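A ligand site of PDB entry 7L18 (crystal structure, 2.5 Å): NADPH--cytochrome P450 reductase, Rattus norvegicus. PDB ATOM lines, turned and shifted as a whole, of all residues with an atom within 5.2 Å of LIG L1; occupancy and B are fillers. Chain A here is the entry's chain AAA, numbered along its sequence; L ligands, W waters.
N of Thr 83 lies within hydrogen-bond range of O of Leu 117. The side-chain hydroxyl of Ser 30 is in hydrogen-bond range of the backbone NH of Thr 34 (3.3 Å). OG of Ser 30 is in hydrogen-bond range of N of Gly 33, 2.7 Å away. The backbone NH (N) of Ser 30 is in hydrogen-bond range of the side-chain hydroxyl (OG1) of Thr 90, at 3.4 Å. OD1 of Asn 126 is in hydrogen-bond range of N of Gly 118 (3.2 Å). N of Leu 117 is in hydrogen-bond range of OD1 of Asn 126 (2.9 Å). N of Asp 152 is in hydrogen-bond range of O of Gly 118, 2.9 Å away. O of Gly 29 sits at hydrogen-bond distance from N of Ala 82.
The backbone carbonyl oxygen (O) of Thr 83 lies within hydrogen-bond range of an oxygen (O3) of LIG L1. N of Thr 34 is in hydrogen-bond range of O7 of LIG L1 (3.0 Å). O7 of LIG L1 is in hydrogen-bond range of OG1 of Thr 34 (2.6 Å). O8 of LIG L1 sits at hydrogen-bond distance from N of Thr 32. An oxygen (O7) of LIG L1 is in hydrogen-bond range of the side-chain hydroxyl (OG1) of Thr 32. An oxygen (O9) of LIG L1 lies within hydrogen-bond range of the side-chain hydroxyl (OG) of Ser 30 (2.8 Å). A nitrogen (N2) of LIG L1 lies within hydrogen-bond range of the backbone carbonyl oxygen (O) of His 124, at 2.8 Å. The backbone NH (N) of Asn 119 sits at hydrogen-bond distance from an oxygen (O1) of LIG L1, at 2.9 Å. The backbone NH (N) of Asn 126 sits at hydrogen-bond distance from an oxygen (O1) of LIG L1 (2.9 Å). The backbone NH of Ala 35 is in hydrogen-bond range of an oxygen (O9) of LIG L1 (2.9 Å). An oxygen (O8) of LIG L1 lies within hydrogen-bond range of the backbone NH (N) of Gln 31 (3.1 Å). The backbone NH of Gly 87 lies within hydrogen-bond range of an oxygen (O2) of LIG L1 (3.2 Å). The backbone NH (N) of Gly 33 sits at hydrogen-bond distance from an oxygen (O7) of LIG L1 (3.3 Å). An oxygen (O3) of LIG L1 sits at hydrogen-bond distance from the backbone carbonyl oxygen (O) of Leu 117, 3.3 Å away.
Water W2 bridges O5 of LIG L1 (2.8 Å) and OG1 of Thr 34 (2.8 Å). Water W1 bridges O8 of LIG L1 and O of Thr 83. Water W3 bridges an oxygen (O8) of LIG L1 (3.0 Å) and the side-chain hydroxyl (OG1) of Thr 32 (3.1 Å).
The backbone carbonyl oxygen (O) of Gly 85 sits close to a nitrogen (N3) of LIG L1, 3.0 Å away. CB of Ala 82 touches O6 of LIG L1, at 3.4 Å. CE1 of Tyr 84 touches C7 of LIG L1, 3.5 Å away. Gly 118 touches LIG L1 (CA to O1, 3.2 Å). Tyr 122 touches LIG L1 (CD2 to N3, 3.4 Å). Phe 125 touches LIG L1 (CA to O1, 3.4 Å). Asp 152 touches LIG L1 (OD2 to O4, 3.7 Å). Leu 156 touches LIG L1. Leu 618 touches LIG L1 (O to C7, 3.5 Å). Hydrophobic or aromatic side chains within 4 Å of LIG L1: Ala 35, Ala 82, Tyr 84, Leu 117, Tyr 122, Phe 125 and Leu 156. Of the 28 residues printed, 21 come within 4 Å of LIG L1. The nearest printed residue that does not touch LIG L1 is Glu 86 (4.1 Å).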
ATOM      1  N   GLY A  29     -25.124  19.876   8.548  1.00  0.00           N
ATOM      2  CA  GLY A  29     -24.632  18.566   8.102  1.00  0.00           C
ATOM      3  C   GLY A  29     -23.269  18.744   7.455  1.00  0.00           C
ATOM      4  O   GLY A  29     -23.242  19.161   6.305  1.00  0.00           O
ATOM      5  N   SER A  30     -22.192  18.477   8.183  1.00  0.00           N
ATOM      6  CA  SER A  30     -20.770  18.781   7.849  1.00  0.00           C
ATOM      7  C   SER A  30     -19.850  17.598   8.208  1.00  0.00           C
ATOM      8  O   SER A  30     -19.836  17.171   9.392  1.00  0.00           O
ATOM      9  CB  SER A  30     -20.325  20.043   8.534  1.00  0.00           C
ATOM     10  OG  SER A  30     -19.149  20.572   7.954  1.00  0.00           O
ATOM     11  N   GLN A  31     -19.128  17.082   7.214  1.00  0.00           N
ATOM     12  CA  GLN A  31     -18.008  16.113   7.411  1.00  0.00           C
ATOM     13  C   GLN A  31     -16.736  16.903   7.702  1.00  0.00           C
ATOM     14  O   GLN A  31     -16.077  16.623   8.733  1.00  0.00           O
ATOM     15  CB  GLN A  31     -17.869  15.196   6.193  1.00  0.00           C
ATOM     16  CG  GLN A  31     -17.210  13.855   6.500  1.00  0.00           C
ATOM     17  CD  GLN A  31     -18.030  12.999   7.435  1.00  0.00           C
ATOM     18  OE1 GLN A  31     -19.263  12.927   7.329  1.00  0.00           O
ATOM     19  NE2 GLN A  31     -17.359  12.320   8.357  1.00  0.00           N
ATOM     20  N   THR A  32     -16.400  17.891   6.864  1.00  0.00           N
ATOM     21  CA  THR A  32     -15.090  18.597   6.926  1.00  0.00           C
ATOM     22  C   THR A  32     -15.259  20.080   7.272  1.00  0.00           C
ATOM     23  O   THR A  32     -14.270  20.825   7.165  1.00  0.00           O
ATOM     24  CB  THR A  32     -14.257  18.305   5.671  1.00  0.00           C
ATOM     25  OG1 THR A  32     -15.097  18.476   4.531  1.00  0.00           O
ATOM     26  CG2 THR A  32     -13.691  16.899   5.678  1.00  0.00           C
ATOM     27  N   GLY A  33     -16.436  20.481   7.756  1.00  0.00           N
ATOM     28  CA  GLY A  33     -16.610  21.765   8.463  1.00  0.00           C
ATOM     29  C   GLY A  33     -17.000  22.917   7.555  1.00  0.00           C
ATOM     30  O   GLY A  33     -17.075  24.039   8.082  1.00  0.00           O
ATOM     31  N   THR A  34     -17.252  22.703   6.256  1.00  0.00           N
ATOM     32  CA  THR A  34     -17.678  23.806   5.346  1.00  0.00           C
ATOM     33  C   THR A  34     -19.131  24.213   5.656  1.00  0.00           C
ATOM     34  O   THR A  34     -19.355  25.412   5.847  1.00  0.00           O
ATOM     35  CB  THR A  34     -17.523  23.499   3.860  1.00  0.00           C
ATOM     36  OG1 THR A  34     -16.290  22.812   3.641  1.00  0.00           O
ATOM     37  CG2 THR A  34     -17.515  24.765   3.017  1.00  0.00           C
ATOM     38  N   ALA A  35     -20.063  23.261   5.734  1.00  0.00           N
ATOM     39  CA  ALA A  35     -21.479  23.536   6.084  1.00  0.00           C
ATOM     40  C   ALA A  35     -21.550  24.160   7.487  1.00  0.00           C
ATOM     41  O   ALA A  35     -22.381  25.082   7.703  1.00  0.00           O
ATOM     42  CB  ALA A  35     -22.309  22.287   5.980  1.00  0.00           C
ATOM     43  N   GLU A  36     -20.696  23.703   8.409  1.00  0.00           N
ATOM     44  CA  GLU A  36     -20.587  24.269   9.786  1.00  0.00           C
ATOM     45  C   GLU A  36     -20.201  25.755   9.691  1.00  0.00           C
ATOM     46  O   GLU A  36     -20.859  26.565  10.358  1.00  0.00           O
ATOM     47  CB  GLU A  36     -19.578  23.476  10.620  1.00  0.00           C
ATOM     48  CG  GLU A  36     -19.221  24.130  11.950  1.00  0.00           C
ATOM     49  CD  GLU A  36     -18.417  23.284  12.922  1.00  0.00           C
ATOM     50  OE1 GLU A  36     -18.160  23.776  14.037  1.00  0.00           O
ATOM     51  OE2 GLU A  36     -18.052  22.138  12.574  1.00  0.00           O
ATOM     52  N   ALA A  82     -24.287  19.408   3.651  1.00  0.00           N
ATOM     53  CA  ALA A  82     -23.270  18.776   2.787  1.00  0.00           C
ATOM     54  C   ALA A  82     -23.735  17.366   2.379  1.00  0.00           C
ATOM     55  O   ALA A  82     -24.412  16.707   3.159  1.00  0.00           O
ATOM     56  CB  ALA A  82     -21.926  18.711   3.478  1.00  0.00           C
ATOM     57  N   THR A  83     -23.381  16.957   1.183  1.00  0.00           N
ATOM     58  CA  THR A  83     -23.559  15.571   0.695  1.00  0.00           C
ATOM     59  C   THR A  83     -22.184  14.877   0.695  1.00  0.00           C
ATOM     60  O   THR A  83     -21.197  15.457   0.159  1.00  0.00           O
ATOM     61  CB  THR A  83     -24.285  15.562  -0.661  1.00  0.00           C
ATOM     62  OG1 THR A  83     -25.569  16.164  -0.487  1.00  0.00           O
ATOM     63  CG2 THR A  83     -24.431  14.171  -1.213  1.00  0.00           C
ATOM     64  N   TYR A  84     -22.129  13.682   1.294  1.00  0.00           N
ATOM     65  CA  TYR A  84     -20.896  12.869   1.459  1.00  0.00           C
ATOM     66  C   TYR A  84     -21.206  11.460   0.948  1.00  0.00           C
ATOM     67  O   TYR A  84     -22.410  11.161   0.734  1.00  0.00           O
ATOM     68  CB  TYR A  84     -20.430  12.919   2.914  1.00  0.00           C
ATOM     69  CG  TYR A  84     -19.024  12.444   3.176  1.00  0.00           C
ATOM     70  CD1 TYR A  84     -17.919  13.098   2.643  1.00  0.00           C
ATOM     71  CD2 TYR A  84     -18.774  11.328   3.966  1.00  0.00           C
ATOM     72  CE1 TYR A  84     -16.627  12.658   2.878  1.00  0.00           C
ATOM     73  CE2 TYR A  84     -17.491  10.871   4.201  1.00  0.00           C
ATOM     74  CZ  TYR A  84     -16.411  11.538   3.659  1.00  0.00           C
ATOM     75  OH  TYR A  84     -15.146  11.100   3.907  1.00  0.00           O
ATOM     76  N   GLY A  85     -20.172  10.648   0.711  1.00  0.00           N
ATOM     77  CA  GLY A  85     -20.300   9.247   0.260  1.00  0.00           C
ATOM     78  C   GLY A  85     -20.917   9.161  -1.117  1.00  0.00           C
ATOM     79  O   GLY A  85     -20.553   9.967  -1.995  1.00  0.00           O
ATOM     80  N   GLU A  86     -21.843   8.218  -1.311  1.00  0.00           N
ATOM     81  CA  GLU A  86     -22.515   7.991  -2.632  1.00  0.00           C
ATOM     82  C   GLU A  86     -23.927   8.580  -2.513  1.00  0.00           C
ATOM     83  O   GLU A  86     -24.924   7.829  -2.628  1.00  0.00           O
ATOM     84  CB  GLU A  86     -22.410   6.507  -2.996  1.00  0.00           C
ATOM     85  CG  GLU A  86     -20.968   5.992  -3.064  1.00  0.00           C
ATOM     86  CD  GLU A  86     -20.718   4.532  -2.667  1.00  0.00           C
ATOM     87  OE1 GLU A  86     -20.839   4.195  -1.471  1.00  0.00           O
ATOM     88  OE2 GLU A  86     -20.391   3.721  -3.564  1.00  0.00           O
ATOM     89  N   GLY A  87     -23.999   9.892  -2.221  1.00  0.00           N
ATOM     90  CA  GLY A  87     -25.268  10.643  -2.042  1.00  0.00           C
ATOM     91  C   GLY A  87     -25.931  10.411  -0.688  1.00  0.00           C
ATOM     92  O   GLY A  87     -27.179  10.581  -0.602  1.00  0.00           O
ATOM     93  N   ASP A  88     -25.121  10.066   0.321  1.00  0.00           N
ATOM     94  CA  ASP A  88     -25.566   9.814   1.729  1.00  0.00           C
ATOM     95  C   ASP A  88     -25.522  11.121   2.515  1.00  0.00           C
ATOM     96  O   ASP A  88     -24.889  12.091   2.078  1.00  0.00           O
ATOM     97  CB  ASP A  88     -24.640   8.806   2.421  1.00  0.00           C
ATOM     98  CG  ASP A  88     -24.627   7.424   1.798  1.00  0.00           C
ATOM     99  OD1 ASP A  88     -25.709   6.828   1.712  1.00  0.00           O
ATOM    100  OD2 ASP A  88     -23.539   6.978   1.400  1.00  0.00           O
ATOM    101  N   THR A  90     -23.963  13.367   5.631  1.00  0.00           N
ATOM    102  CA  THR A  90     -22.767  13.499   6.494  1.00  0.00           C
ATOM    103  C   THR A  90     -23.020  12.659   7.744  1.00  0.00           C
ATOM    104  O   THR A  90     -24.220  12.444   8.075  1.00  0.00           O
ATOM    105  CB  THR A  90     -22.510  14.970   6.846  1.00  0.00           C
ATOM    106  OG1 THR A  90     -23.708  15.515   7.430  1.00  0.00           O
ATOM    107  CG2 THR A  90     -22.103  15.778   5.645  1.00  0.00           C
ATOM    108  N   LEU A 117     -24.702  21.806   0.123  1.00  0.00           N
ATOM    109  CA  LEU A 117     -23.281  21.774  -0.290  1.00  0.00           C
ATOM    110  C   LEU A 117     -23.028  20.474  -1.046  1.00  0.00           C
ATOM    111  O   LEU A 117     -23.199  19.393  -0.442  1.00  0.00           O
ATOM    112  CB  LEU A 117     -22.349  21.859   0.925  1.00  0.00           C
ATOM    113  CG  LEU A 117     -22.282  23.199   1.629  1.00  0.00           C
ATOM    114  CD1 LEU A 117     -23.457  23.374   2.584  1.00  0.00           C
ATOM    115  CD2 LEU A 117     -20.970  23.341   2.377  1.00  0.00           C
ATOM    116  N   GLY A 118     -22.634  20.561  -2.309  1.00  0.00           N
ATOM    117  CA  GLY A 118     -22.431  19.353  -3.123  1.00  0.00           C
ATOM    118  C   GLY A 118     -21.320  19.559  -4.118  1.00  0.00           C
ATOM    119  O   GLY A 118     -20.614  20.568  -4.005  1.00  0.00           O
ATOM    120  N   ASN A 119     -21.224  18.652  -5.097  1.00  0.00           N
ATOM    121  CA  ASN A 119     -20.225  18.724  -6.199  1.00  0.00           C
ATOM    122  C   ASN A 119     -20.771  18.030  -7.452  1.00  0.00           C
ATOM    123  O   ASN A 119     -21.103  16.842  -7.382  1.00  0.00           O
ATOM    124  CB  ASN A 119     -18.905  18.134  -5.725  1.00  0.00           C
ATOM    125  CG  ASN A 119     -17.812  18.305  -6.751  1.00  0.00           C
ATOM    126  OD1 ASN A 119     -18.017  18.032  -7.935  1.00  0.00           O
ATOM    127  ND2 ASN A 119     -16.657  18.773  -6.292  1.00  0.00           N
ATOM    128  N   TYR A 122     -19.848  14.480  -8.873  1.00  0.00           N
ATOM    129  CA  TYR A 122     -20.434  13.305  -8.164  1.00  0.00           C
ATOM    130  C   TYR A 122     -21.811  12.972  -8.736  1.00  0.00           C
ATOM    131  O   TYR A 122     -22.604  13.878  -9.084  1.00  0.00           O
ATOM    132  CB  TYR A 122     -20.501  13.545  -6.654  1.00  0.00           C
ATOM    133  CG  TYR A 122     -19.158  13.470  -5.973  1.00  0.00           C
ATOM    134  CD1 TYR A 122     -18.314  14.567  -5.959  1.00  0.00           C
ATOM    135  CD2 TYR A 122     -18.707  12.310  -5.382  1.00  0.00           C
ATOM    136  CE1 TYR A 122     -17.071  14.520  -5.352  1.00  0.00           C
ATOM    137  CE2 TYR A 122     -17.460  12.238  -4.791  1.00  0.00           C
ATOM    138  CZ  TYR A 122     -16.633  13.356  -4.764  1.00  0.00           C
ATOM    139  OH  TYR A 122     -15.400  13.291  -4.188  1.00  0.00           O
ATOM    140  N   HIS A 124     -24.571  11.850  -7.440  1.00  0.00           N
ATOM    141  CA  HIS A 124     -25.736  12.310  -6.637  1.00  0.00           C
ATOM    142  C   HIS A 124     -25.493  13.754  -6.149  1.00  0.00           C
ATOM    143  O   HIS A 124     -25.184  13.940  -4.956  1.00  0.00           O
ATOM    144  CB  HIS A 124     -26.010  11.346  -5.471  1.00  0.00           C
ATOM    145  CG  HIS A 124     -26.217   9.918  -5.836  1.00  0.00           C
ATOM    146  ND1 HIS A 124     -27.459   9.426  -6.254  1.00  0.00           N
ATOM    147  CD2 HIS A 124     -25.378   8.856  -5.810  1.00  0.00           C
ATOM    148  CE1 HIS A 124     -27.355   8.131  -6.476  1.00  0.00           C
ATOM    149  NE2 HIS A 124     -26.088   7.760  -6.204  1.00  0.00           N
ATOM    150  N   PHE A 125     -25.613  14.726  -7.050  1.00  0.00           N
ATOM    151  CA  PHE A 125     -25.336  16.164  -6.803  1.00  0.00           C
ATOM    152  C   PHE A 125     -26.331  16.706  -5.764  1.00  0.00           C
ATOM    153  O   PHE A 125     -27.530  16.808  -6.084  1.00  0.00           O
ATOM    154  CB  PHE A 125     -25.387  16.979  -8.093  1.00  0.00           C
ATOM    155  CG  PHE A 125     -25.225  18.465  -7.885  1.00  0.00           C
ATOM    156  CD1 PHE A 125     -24.066  18.964  -7.292  1.00  0.00           C
ATOM    157  CD2 PHE A 125     -26.232  19.355  -8.217  1.00  0.00           C
ATOM    158  CE1 PHE A 125     -23.915  20.321  -7.069  1.00  0.00           C
ATOM    159  CE2 PHE A 125     -26.076  20.709  -7.982  1.00  0.00           C
ATOM    160  CZ  PHE A 125     -24.912  21.195  -7.418  1.00  0.00           C
ATOM    161  N   ASN A 126     -25.841  17.047  -4.562  1.00  0.00           N
ATOM    162  CA  ASN A 126     -26.636  17.623  -3.440  1.00  0.00           C
ATOM    163  C   ASN A 126     -27.862  16.739  -3.129  1.00  0.00           C
ATOM    164  O   ASN A 126     -28.931  17.310  -2.806  1.00  0.00           O
ATOM    165  CB  ASN A 126     -27.064  19.061  -3.727  1.00  0.00           C
ATOM    166  CG  ASN A 126     -26.072  20.058  -3.176  1.00  0.00           C
ATOM    167  OD1 ASN A 126     -25.831  20.100  -1.961  1.00  0.00           O
ATOM    168  ND2 ASN A 126     -25.486  20.842  -4.052  1.00  0.00           N
ATOM    169  N   ALA A 127     -27.715  15.410  -3.188  1.00  0.00           N
ATOM    170  CA  ALA A 127     -28.785  14.459  -2.813  1.00  0.00           C
ATOM    171  C   ALA A 127     -29.390  14.892  -1.471  1.00  0.00           C
ATOM    172  O   ALA A 127     -30.623  14.887  -1.346  1.00  0.00           O
ATOM    173  CB  ALA A 127     -28.258  13.050  -2.733  1.00  0.00           C
ATOM    174  N   ASP A 152     -18.970  22.634  -5.242  1.00  0.00           N
ATOM    175  CA  ASP A 152     -17.510  22.737  -4.971  1.00  0.00           C
ATOM    176  C   ASP A 152     -16.728  22.606  -6.284  1.00  0.00           C
ATOM    177  O   ASP A 152     -15.604  23.103  -6.329  1.00  0.00           O
ATOM    178  CB  ASP A 152     -17.032  21.718  -3.921  1.00  0.00           C
ATOM    179  CG  ASP A 152     -15.753  22.145  -3.200  1.00  0.00           C
ATOM    180  OD1 ASP A 152     -15.627  23.357  -2.850  1.00  0.00           O
ATOM    181  OD2 ASP A 152     -14.879  21.278  -2.992  1.00  0.00           O
ATOM    182  N   LEU A 156     -17.939  27.162  -4.495  1.00  0.00           N
ATOM    183  CA  LEU A 156     -18.977  26.953  -3.448  1.00  0.00           C
ATOM    184  C   LEU A 156     -19.161  28.241  -2.640  1.00  0.00           C
ATOM    185  O   LEU A 156     -20.342  28.656  -2.390  1.00  0.00           O
ATOM    186  CB  LEU A 156     -18.527  25.793  -2.554  1.00  0.00           C
ATOM    187  CG  LEU A 156     -19.504  25.362  -1.460  1.00  0.00           C
ATOM    188  CD1 LEU A 156     -20.865  24.998  -2.024  1.00  0.00           C
ATOM    189  CD2 LEU A 156     -18.942  24.191  -0.669  1.00  0.00           C
ATOM    190  N   LEU A 618     -14.455   7.169  -4.097  1.00  0.00           N
ATOM    191  CA  LEU A 618     -13.944   8.326  -4.888  1.00  0.00           C
ATOM    192  C   LEU A 618     -13.555   9.504  -3.997  1.00  0.00           C
ATOM    193  O   LEU A 618     -14.202   9.702  -2.939  1.00  0.00           O
ATOM    194  CB  LEU A 618     -15.011   8.745  -5.895  1.00  0.00           C
ATOM    195  CG  LEU A 618     -15.453   7.662  -6.866  1.00  0.00           C
ATOM    196  CD1 LEU A 618     -16.577   8.188  -7.758  1.00  0.00           C
ATOM    197  CD2 LEU A 618     -14.282   7.165  -7.705  1.00  0.00           C
ATOM    198  N   TRP A 619     -12.562  10.282  -4.433  1.00  0.00           N
ATOM    199  CA  TRP A 619     -12.139  11.566  -3.820  1.00  0.00           C
ATOM    200  C   TRP A 619     -11.444  12.441  -4.876  1.00  0.00           C
ATOM    201  O   TRP A 619     -10.952  11.884  -5.876  1.00  0.00           O
ATOM    202  CB  TRP A 619     -11.251  11.326  -2.583  1.00  0.00           C
ATOM    203  CG  TRP A 619      -9.844  10.897  -2.893  1.00  0.00           C
ATOM    204  CD1 TRP A 619      -8.798  11.704  -3.202  1.00  0.00           C
ATOM    205  CD2 TRP A 619      -9.345   9.548  -2.913  1.00  0.00           C
ATOM    206  NE1 TRP A 619      -7.668  10.956  -3.420  1.00  0.00           N
ATOM    207  CE2 TRP A 619      -7.972   9.630  -3.261  1.00  0.00           C
ATOM    208  CE3 TRP A 619      -9.895   8.279  -2.673  1.00  0.00           C
ATOM    209  CZ2 TRP A 619      -7.168   8.497  -3.371  1.00  0.00           C
ATOM    210  CZ3 TRP A 619      -9.097   7.160  -2.777  1.00  0.00           C
ATOM    211  CH2 TRP A 619      -7.744   7.274  -3.124  1.00  0.00           C
HETATM  212  N1  LIG L   1     -21.079  16.084  -3.289  1.00  0.00           N
HETATM  213  C1  LIG L   1     -22.227  15.658  -3.878  1.00  0.00           C
HETATM  214  O1  LIG L   1     -23.000  16.465  -4.395  1.00  0.00           O
HETATM  215  N2  LIG L   1     -22.587  14.339  -3.882  1.00  0.00           N
HETATM  216  C2  LIG L   1     -21.803  13.370  -3.297  1.00  0.00           C
HETATM  217  O2  LIG L   1     -22.168  12.199  -3.344  1.00  0.00           O
HETATM  218  C3  LIG L   1     -20.569  13.764  -2.732  1.00  0.00           C
HETATM  219  N3  LIG L   1     -19.792  12.854  -2.210  1.00  0.00           N
HETATM  220  C4  LIG L   1     -18.584  13.262  -1.717  1.00  0.00           C
HETATM  221  C5  LIG L   1     -17.726  12.267  -1.213  1.00  0.00           C
HETATM  222  C6  LIG L   1     -16.482  12.579  -0.727  1.00  0.00           C
HETATM  223  C7  LIG L   1     -15.602  11.472  -0.212  1.00  0.00           C
HETATM  224  C8  LIG L   1     -16.050  13.940  -0.699  1.00  0.00           C
HETATM  225  C9  LIG L   1     -14.697  14.319  -0.160  1.00  0.00           C
HETATM  226  C10 LIG L   1     -16.906  14.923  -1.159  1.00  0.00           C
HETATM  227  C11 LIG L   1     -18.167  14.609  -1.701  1.00  0.00           C
HETATM  228  N4  LIG L   1     -19.051  15.572  -2.208  1.00  0.00           N
HETATM  229  C12 LIG L   1     -20.264  15.178  -2.767  1.00  0.00           C
HETATM  230  C13 LIG L   1     -18.675  17.007  -2.215  1.00  0.00           C
HETATM  231  C14 LIG L   1     -18.912  17.669  -0.854  1.00  0.00           C
HETATM  232  O3  LIG L   1     -20.310  17.723  -0.542  1.00  0.00           O
HETATM  233  C15 LIG L   1     -18.359  19.092  -0.779  1.00  0.00           C
HETATM  234  O4  LIG L   1     -16.933  19.090  -0.796  1.00  0.00           O
HETATM  235  C16 LIG L   1     -18.833  19.852   0.461  1.00  0.00           C
HETATM  236  O5  LIG L   1     -18.388  21.207   0.379  1.00  0.00           O
HETATM  237  C17 LIG L   1     -18.311  19.247   1.750  1.00  0.00           C
HETATM  238  O6  LIG L   1     -18.817  20.047   2.838  1.00  0.00           O
HETATM  239  P1  LIG L   1     -18.299  19.778   4.321  1.00  0.00           P
HETATM  240  O7  LIG L   1     -16.924  20.384   4.456  1.00  0.00           O
HETATM  241  O8  LIG L   1     -18.351  18.270   4.503  1.00  0.00           O
HETATM  242  O9  LIG L   1     -19.293  20.511   5.198  1.00  0.00           O
HETATM  243  P1  LG2 L   2      -4.109  19.778   1.869  1.00  0.00           P
HETATM  244  O1  LG2 L   2      -3.119  20.653   2.551  1.00  0.00           O
HETATM  245  O2  LG2 L   2      -5.426  19.487   2.492  1.00  0.00           O
HETATM  246  O3  LG2 L   2      -4.338  20.325   0.398  1.00  0.00           O
HETATM  247  C1  LG2 L   2      -5.343  19.749  -0.445  1.00  0.00           C
HETATM  248  C2  LG2 L   2      -5.630  20.750  -1.533  1.00  0.00           C
HETATM  249  O4  LG2 L   2      -4.414  21.047  -2.258  1.00  0.00           O
HETATM  250  C3  LG2 L   2      -6.593  20.311  -2.634  1.00  0.00           C
HETATM  251  O5  LG2 L   2      -7.947  20.432  -2.214  1.00  0.00           O
HETATM  252  C4  LG2 L   2      -6.258  21.334  -3.718  1.00  0.00           C
HETATM  253  O6  LG2 L   2      -6.978  22.525  -3.529  1.00  0.00           O
HETATM  254  C5  LG2 L   2      -4.777  21.628  -3.499  1.00  0.00           C
HETATM  255  N1  LG2 L   2      -3.892  21.130  -4.564  1.00  0.00           N
HETATM  256  C6  LG2 L   2      -3.237  19.904  -4.683  1.00  0.00           C
HETATM  257  N2  LG2 L   2      -2.493  19.836  -5.764  1.00  0.00           N
HETATM  258  C7  LG2 L   2      -2.661  21.066  -6.389  1.00  0.00           C
HETATM  259  C8  LG2 L   2      -2.138  21.625  -7.576  1.00  0.00           C
HETATM  260  N3  LG2 L   2      -1.276  20.992  -8.368  1.00  0.00           N
HETATM  261  N4  LG2 L   2      -2.514  22.880  -7.907  1.00  0.00           N
HETATM  262  C9  LG2 L   2      -3.369  23.520  -7.093  1.00  0.00           C
HETATM  263  N5  LG2 L   2      -3.918  23.109  -5.955  1.00  0.00           N
HETATM  264  C10 LG2 L   2      -3.513  21.862  -5.659  1.00  0.00           C
HETATM  265  N6  LG2 L   2      -5.117  10.519  -0.442  1.00  0.00           N
HETATM  266  C11 LG2 L   2      -4.190   9.638  -0.741  1.00  0.00           C
HETATM  267  O7  LG2 L   2      -3.086  10.001  -1.120  1.00  0.00           O
HETATM  268  N7  LG2 L   2      -4.406   8.290  -0.596  1.00  0.00           N
HETATM  269  C12 LG2 L   2      -5.597   7.780  -0.179  1.00  0.00           C
HETATM  270  O8  LG2 L   2      -5.738   6.574  -0.043  1.00  0.00           O
HETATM  271  C13 LG2 L   2      -6.634   8.705   0.093  1.00  0.00           C
HETATM  272  N8  LG2 L   2      -7.822   8.273   0.447  1.00  0.00           N
HETATM  273  C14 LG2 L   2      -8.796   9.199   0.674  1.00  0.00           C
HETATM  274  C15 LG2 L   2     -10.077   8.758   1.045  1.00  0.00           C
HETATM  275  C16 LG2 L   2     -11.097   9.640   1.308  1.00  0.00           C
HETATM  276  C17 LG2 L   2     -12.448   9.122   1.732  1.00  0.00           C
HETATM  277  C18 LG2 L   2     -10.856  11.042   1.203  1.00  0.00           C
HETATM  278  C19 LG2 L   2     -11.946  12.051   1.481  1.00  0.00           C
HETATM  279  C20 LG2 L   2      -9.606  11.478   0.846  1.00  0.00           C
HETATM  280  C21 LG2 L   2      -8.564  10.584   0.570  1.00  0.00           C
HETATM  281  N9  LG2 L   2      -7.293  10.997   0.190  1.00  0.00           N
HETATM  282  C22 LG2 L   2      -6.287  10.088  -0.073  1.00  0.00           C
HETATM  283  C23 LG2 L   2      -6.983  12.443   0.120  1.00  0.00           C
HETATM  284  C24 LG2 L   2      -6.593  12.923   1.505  1.00  0.00           C
HETATM  285  O9  LG2 L   2      -7.748  12.964   2.380  1.00  0.00           O
HETATM  286  C25 LG2 L   2      -5.890  14.282   1.495  1.00  0.00           C
HETATM  287  O10 LG2 L   2      -6.738  15.283   0.972  1.00  0.00           O
HETATM  288  C26 LG2 L   2      -4.588  14.346   0.689  1.00  0.00           C
HETATM  289  O11 LG2 L   2      -3.628  13.400   1.174  1.00  0.00           O
HETATM  290  C27 LG2 L   2      -3.988  15.723   0.763  1.00  0.00           C
HETATM  291  O12 LG2 L   2      -4.110  16.226   2.137  1.00  0.00           O
HETATM  292  P2  LG2 L   2      -3.003  17.256   2.642  1.00  0.00           P
HETATM  293  O13 LG2 L   2      -1.634  16.712   2.442  1.00  0.00           O
HETATM  294  O14 LG2 L   2      -3.362  17.633   4.040  1.00  0.00           O
HETATM  295  O15 LG2 L   2      -3.333  18.413   1.604  1.00  0.00           O
HETATM  296  O   HOH W   1     -19.239  15.980   2.965  1.00  0.00           O
HETATM  297  O   HOH W   2     -16.058  22.628   0.839  1.00  0.00           O
HETATM  298  O   HOH W   3     -16.698  16.402   2.857  1.00  0.00           O
